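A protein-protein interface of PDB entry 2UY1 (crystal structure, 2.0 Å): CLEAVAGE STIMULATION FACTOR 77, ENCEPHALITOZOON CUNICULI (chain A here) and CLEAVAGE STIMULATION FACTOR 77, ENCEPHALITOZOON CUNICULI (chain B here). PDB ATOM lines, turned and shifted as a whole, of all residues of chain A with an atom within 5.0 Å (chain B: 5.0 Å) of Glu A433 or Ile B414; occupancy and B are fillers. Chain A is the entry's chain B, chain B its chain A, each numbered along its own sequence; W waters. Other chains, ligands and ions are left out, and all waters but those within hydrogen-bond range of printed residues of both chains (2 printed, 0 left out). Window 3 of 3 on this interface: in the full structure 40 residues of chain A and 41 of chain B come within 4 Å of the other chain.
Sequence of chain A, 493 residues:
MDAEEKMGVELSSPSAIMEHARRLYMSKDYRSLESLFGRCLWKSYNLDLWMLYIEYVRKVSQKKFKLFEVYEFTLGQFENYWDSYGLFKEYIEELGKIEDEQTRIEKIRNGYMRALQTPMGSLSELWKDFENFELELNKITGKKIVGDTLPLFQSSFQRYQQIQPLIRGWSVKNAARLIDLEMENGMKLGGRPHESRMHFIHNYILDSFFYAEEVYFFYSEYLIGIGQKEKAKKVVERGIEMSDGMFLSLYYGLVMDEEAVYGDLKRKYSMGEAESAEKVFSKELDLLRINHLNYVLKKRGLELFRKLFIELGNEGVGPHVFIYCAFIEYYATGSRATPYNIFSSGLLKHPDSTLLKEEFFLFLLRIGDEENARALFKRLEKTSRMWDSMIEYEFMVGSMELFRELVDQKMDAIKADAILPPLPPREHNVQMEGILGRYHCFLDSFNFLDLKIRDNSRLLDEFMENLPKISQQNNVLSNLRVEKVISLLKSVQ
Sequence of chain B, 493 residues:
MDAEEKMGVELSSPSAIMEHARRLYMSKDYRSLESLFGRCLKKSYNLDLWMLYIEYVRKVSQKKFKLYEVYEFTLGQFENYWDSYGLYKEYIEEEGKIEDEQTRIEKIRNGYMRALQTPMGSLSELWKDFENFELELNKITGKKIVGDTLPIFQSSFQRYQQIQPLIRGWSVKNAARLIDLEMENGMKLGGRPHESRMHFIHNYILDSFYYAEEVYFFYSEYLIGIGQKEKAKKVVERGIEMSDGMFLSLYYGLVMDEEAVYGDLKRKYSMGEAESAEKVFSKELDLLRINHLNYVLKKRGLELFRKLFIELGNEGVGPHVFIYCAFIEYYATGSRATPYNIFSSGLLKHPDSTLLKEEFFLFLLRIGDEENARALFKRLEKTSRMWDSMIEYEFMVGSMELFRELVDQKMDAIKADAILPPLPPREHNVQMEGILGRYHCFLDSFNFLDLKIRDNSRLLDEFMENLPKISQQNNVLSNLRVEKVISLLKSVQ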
ATOM      1  N   ASP A 180      10.361   6.177 -35.807  1.00  0.00           N
ATOM      2  CA  ASP A 180      10.287   6.276 -34.330  1.00  0.00           C
ATOM      3  C   ASP A 180       9.740   5.009 -33.643  1.00  0.00           C
ATOM      4  O   ASP A 180      10.291   4.564 -32.649  1.00  0.00           O
ATOM      5  CB  ASP A 180       9.431   7.468 -33.908  1.00  0.00           C
ATOM      6  CG  ASP A 180       9.978   8.805 -34.375  1.00  0.00           C
ATOM      7  OD1 ASP A 180      11.218   9.035 -34.335  1.00  0.00           O
ATOM      8  OD2 ASP A 180       9.133   9.637 -34.785  1.00  0.00           O
ATOM      9  N   VAL A 430       7.631  21.032 -27.587  1.00  0.00           N
ATOM     10  CA  VAL A 430       6.746  20.024 -28.129  1.00  0.00           C
ATOM     11  C   VAL A 430       5.816  20.571 -29.209  1.00  0.00           C
ATOM     12  O   VAL A 430       4.580  20.524 -29.016  1.00  0.00           O
ATOM     13  CB  VAL A 430       5.803  19.511 -27.030  1.00  0.00           C
ATOM     14  CG1 VAL A 430       5.011  18.281 -27.477  1.00  0.00           C
ATOM     15  CG2 VAL A 430       6.553  19.255 -25.773  1.00  0.00           C
ATOM     16  N   GLN A 431       6.351  21.102 -30.312  1.00  0.00           N
ATOM     17  CA  GLN A 431       5.544  21.217 -31.537  1.00  0.00           C
ATOM     18  C   GLN A 431       5.608  19.809 -32.161  1.00  0.00           C
ATOM     19  O   GLN A 431       4.669  19.009 -32.036  1.00  0.00           O
ATOM     20  CB  GLN A 431       6.073  22.315 -32.493  1.00  0.00           C
ATOM     21  CG  GLN A 431       5.109  22.724 -33.635  1.00  0.00           C
ATOM     22  CD  GLN A 431       4.564  24.184 -33.561  1.00  0.00           C
ATOM     23  OE1 GLN A 431       5.131  25.014 -32.687  1.00  0.00           O
ATOM     24  NE2 GLN A 431       3.651  24.540 -34.305  1.00  0.00           N
ATOM     25  N   MET A 432       6.740  19.511 -32.794  1.00  0.00           N
ATOM     26  CA  MET A 432       7.050  18.193 -33.314  1.00  0.00           C
ATOM     27  C   MET A 432       7.874  17.306 -32.329  1.00  0.00           C
ATOM     28  O   MET A 432       8.583  17.785 -31.435  1.00  0.00           O
ATOM     29  CB  MET A 432       7.742  18.307 -34.681  1.00  0.00           C
ATOM     30  CG  MET A 432       6.966  19.102 -35.774  1.00  0.00           C
ATOM     31  SD  MET A 432       5.232  18.580 -35.947  1.00  0.00           S
ATOM     32  CE  MET A 432       4.518  20.057 -36.748  1.00  0.00           C
ATOM     33  N   GLU A 433       7.741  16.006 -32.546  1.00  0.00           N
ATOM     34  CA  GLU A 433       8.244  14.939 -31.710  1.00  0.00           C
ATOM     35  C   GLU A 433       9.119  13.920 -32.509  1.00  0.00           C
ATOM     36  O   GLU A 433       9.042  13.864 -33.708  1.00  0.00           O
ATOM     37  CB  GLU A 433       7.033  14.191 -31.128  1.00  0.00           C
ATOM     38  CG  GLU A 433       7.507  12.940 -30.434  1.00  0.00           C
ATOM     39  CD  GLU A 433       6.510  12.179 -29.588  1.00  0.00           C
ATOM     40  OE1 GLU A 433       5.291  12.539 -29.566  1.00  0.00           O
ATOM     41  OE2 GLU A 433       7.018  11.211 -28.944  1.00  0.00           O
ATOM     42  N   GLY A 434       9.903  13.074 -31.848  1.00  0.00           N
ATOM     43  CA  GLY A 434      10.678  12.030 -32.557  1.00  0.00           C
ATOM     44  C   GLY A 434      11.684  12.605 -33.555  1.00  0.00           C
ATOM     45  O   GLY A 434      12.261  13.664 -33.310  1.00  0.00           O
ATOM     46  N   ILE A 435      11.897  11.922 -34.691  1.00  0.00           N
ATOM     47  CA  ILE A 435      12.945  12.342 -35.616  1.00  0.00           C
ATOM     48  C   ILE A 435      12.564  13.588 -36.451  1.00  0.00           C
ATOM     49  O   ILE A 435      13.443  14.363 -36.902  1.00  0.00           O
ATOM     50  CB  ILE A 435      13.482  11.152 -36.493  1.00  0.00           C
ATOM     51  CG1 ILE A 435      14.736  11.597 -37.263  1.00  0.00           C
ATOM     52  CG2 ILE A 435      12.361  10.581 -37.392  1.00  0.00           C
ATOM     53  CD1 ILE A 435      16.028  11.520 -36.450  1.00  0.00           C
ATOM     54  N   LEU A 436      11.268  13.810 -36.642  1.00  0.00           N
ATOM     55  CA  LEU A 436      10.816  15.075 -37.253  1.00  0.00           C
ATOM     56  C   LEU A 436      10.966  16.271 -36.288  1.00  0.00           C
ATOM     57  O   LEU A 436      11.310  17.347 -36.684  1.00  0.00           O
ATOM     58  CB  LEU A 436       9.365  14.929 -37.706  1.00  0.00           C
ATOM     59  CG  LEU A 436       8.661  15.989 -38.569  1.00  0.00           C
ATOM     60  CD1 LEU A 436       9.432  16.399 -39.811  1.00  0.00           C
ATOM     61  CD2 LEU A 436       7.279  15.480 -38.959  1.00  0.00           C
ATOM     62  N   GLY A 437      10.665  16.045 -35.019  1.00  0.00           N
ATOM     63  CA  GLY A 437      11.073  16.915 -33.915  1.00  0.00           C
ATOM     64  C   GLY A 437      12.514  17.345 -33.997  1.00  0.00           C
ATOM     65  O   GLY A 437      12.817  18.551 -33.923  1.00  0.00           O
ATOM     66  N   LYS B 410      15.123  16.830 -24.816  1.00  0.00           N
ATOM     67  CA  LYS B 410      13.801  17.336 -25.165  1.00  0.00           C
ATOM     68  C   LYS B 410      12.917  16.265 -25.780  1.00  0.00           C
ATOM     69  O   LYS B 410      11.746  16.123 -25.408  1.00  0.00           O
ATOM     70  CB  LYS B 410      13.867  18.513 -26.116  1.00  0.00           C
ATOM     71  CG  LYS B 410      12.468  19.085 -26.257  1.00  0.00           C
ATOM     72  CD  LYS B 410      12.331  20.067 -27.369  1.00  0.00           C
ATOM     73  CE  LYS B 410      11.058  20.878 -27.101  1.00  0.00           C
ATOM     74  NZ  LYS B 410      10.530  21.410 -28.383  1.00  0.00           N
ATOM     75  N   MET B 411      13.454  15.513 -26.731  1.00  0.00           N
ATOM     76  CA  MET B 411      12.673  14.404 -27.315  1.00  0.00           C
ATOM     77  C   MET B 411      12.307  13.388 -26.239  1.00  0.00           C
ATOM     78  O   MET B 411      11.193  12.896 -26.201  1.00  0.00           O
ATOM     79  CB  MET B 411      13.410  13.729 -28.478  1.00  0.00           C
ATOM     80  CG  MET B 411      13.655  14.695 -29.678  1.00  0.00           C
ATOM     81  SD  MET B 411      12.259  15.675 -30.293  1.00  0.00           S
ATOM     82  CE  MET B 411      12.637  17.281 -29.620  1.00  0.00           C
ATOM     83  N   ASP B 412      13.264  13.029 -25.404  1.00  0.00           N
ATOM     84  CA  ASP B 412      12.957  12.129 -24.321  1.00  0.00           C
ATOM     85  C   ASP B 412      11.885  12.699 -23.455  1.00  0.00           C
ATOM     86  O   ASP B 412      11.070  11.946 -22.956  1.00  0.00           O
ATOM     87  CB  ASP B 412      14.160  11.881 -23.425  1.00  0.00           C
ATOM     88  CG  ASP B 412      15.157  10.947 -24.040  1.00  0.00           C
ATOM     89  OD1 ASP B 412      14.824  10.279 -25.066  1.00  0.00           O
ATOM     90  OD2 ASP B 412      16.269  10.913 -23.484  1.00  0.00           O
ATOM     91  N   ALA B 413      11.895  14.026 -23.245  1.00  0.00           N
ATOM     92  CA  ALA B 413      10.928  14.646 -22.312  1.00  0.00           C
ATOM     93  C   ALA B 413       9.516  14.673 -22.864  1.00  0.00           C
ATOM     94  O   ALA B 413       8.552  14.527 -22.093  1.00  0.00           O
ATOM     95  CB  ALA B 413      11.380  16.050 -21.874  1.00  0.00           C
ATOM     96  N   ILE B 414       9.386  14.860 -24.186  1.00  0.00           N
ATOM     97  CA  ILE B 414       8.069  14.926 -24.857  1.00  0.00           C
ATOM     98  C   ILE B 414       7.506  13.519 -24.813  1.00  0.00           C
ATOM     99  O   ILE B 414       6.320  13.343 -24.648  1.00  0.00           O
ATOM    100  CB  ILE B 414       8.161  15.339 -26.390  1.00  0.00           C
ATOM    101  CG1 ILE B 414       8.644  16.798 -26.590  1.00  0.00           C
ATOM    102  CG2 ILE B 414       6.841  15.170 -27.108  1.00  0.00           C
ATOM    103  CD1 ILE B 414       9.108  17.079 -28.036  1.00  0.00           C
ATOM    104  N   LYS B 415       8.375  12.531 -25.000  1.00  0.00           N
ATOM    105  CA  LYS B 415       8.046  11.073 -24.896  1.00  0.00           C
ATOM    106  C   LYS B 415       7.453  10.649 -23.524  1.00  0.00           C
ATOM    107  O   LYS B 415       6.392   9.983 -23.469  1.00  0.00           O
ATOM    108  CB  LYS B 415       9.300  10.246 -25.224  1.00  0.00           C
ATOM    109  CG  LYS B 415       9.098   8.684 -25.272  1.00  0.00           C
ATOM    110  CD  LYS B 415       9.696   8.062 -26.552  1.00  0.00           C
ATOM    111  CE  LYS B 415       8.818   6.878 -27.085  1.00  0.00           C
ATOM    112  NZ  LYS B 415       9.011   6.583 -28.579  1.00  0.00           N
ATOM    113  N   ALA B 416       8.135  11.025 -22.439  1.00  0.00           N
ATOM    114  CA  ALA B 416       7.670  10.780 -21.055  1.00  0.00           C
ATOM    115  C   ALA B 416       6.544  11.725 -20.553  1.00  0.00           C
ATOM    116  O   ALA B 416       6.073  11.602 -19.407  1.00  0.00           O
ATOM    117  CB  ALA B 416       8.846  10.800 -20.102  1.00  0.00           C
ATOM    118  N   ASP B 417       6.074  12.621 -21.423  1.00  0.00           N
ATOM    119  CA  ASP B 417       5.048  13.634 -21.090  1.00  0.00           C
ATOM    120  C   ASP B 417       5.485  14.290 -19.806  1.00  0.00           C
ATOM    121  O   ASP B 417       4.701  14.477 -18.881  1.00  0.00           O
ATOM    122  CB  ASP B 417       3.615  13.071 -21.000  1.00  0.00           C
ATOM    123  CG  ASP B 417       3.039  12.614 -22.364  1.00  0.00           C
ATOM    124  OD1 ASP B 417       3.493  13.072 -23.438  1.00  0.00           O
ATOM    125  OD2 ASP B 417       2.105  11.783 -22.372  1.00  0.00           O
ATOM    126  N   ILE B 419       6.915  17.304 -20.050  1.00  0.00           N
ATOM    127  CA  ILE B 419       6.856  18.723 -20.350  1.00  0.00           C
ATOM    128  C   ILE B 419       5.829  19.456 -19.464  1.00  0.00           C
ATOM    129  O   ILE B 419       4.697  19.003 -19.311  1.00  0.00           O
ATOM    130  CB  ILE B 419       6.525  19.001 -21.825  1.00  0.00           C
ATOM    131  CG1 ILE B 419       7.447  18.220 -22.796  1.00  0.00           C
ATOM    132  CG2 ILE B 419       6.571  20.549 -22.143  1.00  0.00           C
ATOM    133  CD1 ILE B 419       8.712  18.897 -23.113  1.00  0.00           C
HETATM  134  O   HOH W   1      10.036  12.731 -28.869  1.00  0.00           O
HETATM  135  O   HOH W   2      10.305  19.917 -30.393  1.00  0.00           O
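Among the printed residues, merely in contact across the chains: Val A430 with Ile B419, Val A430 with Ile B414, Met A432 with Ile B414 and Glu A433 with Ile B414.
Printed residues of chain B within 4 Å of Val A430: Lys B410, Ile B414 and Ile B419. Of the printed residues of chain B, Glu A433 touches Ile B414. Of the printed residues of chain B, Gly A434 touches Met B411. Of the printed residues of chain A, Lys B410 touches Val A430. Of the printed residues of chain A, Met B411 touches Gly A434 (3.6 Å). Ile B414 touches three residues of chain A. Of the printed residues of chain A, Ile B419 touches Val A430 (3.3 Å). The nearest printed residue of chain B that does not touch Met A432 is Met B411 (4.4 Å).
Water W2 bridges NZ of Lys B410 (2.5 Å) and O of Met A432 (2.9 Å). Water W1 lies within hydrogen-bond range of O of Met B411 (2.9 Å), N of Gly A434 (3.0 Å) and OE2 of Glu A433 (3.4 Å).
The backbone carbonyl oxygen (O) of Gly A434 lies close to the side-chain sulfur (SD) of Met B411, 3.6 Å away. The backbone NH (N) of Val A430 lies close to the side-chain amino group (NZ) of Lys B410 (3.0 Å).
Of the 9 printed residues of chain B, 4 touch a printed residue of chain A. Among the printed residues, 6 pairs touch across the chains. Among the printed residues, no Asp or Glu carboxylate lies within 4 Å of a Lys or Arg side-chain nitrogen of the other chain.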
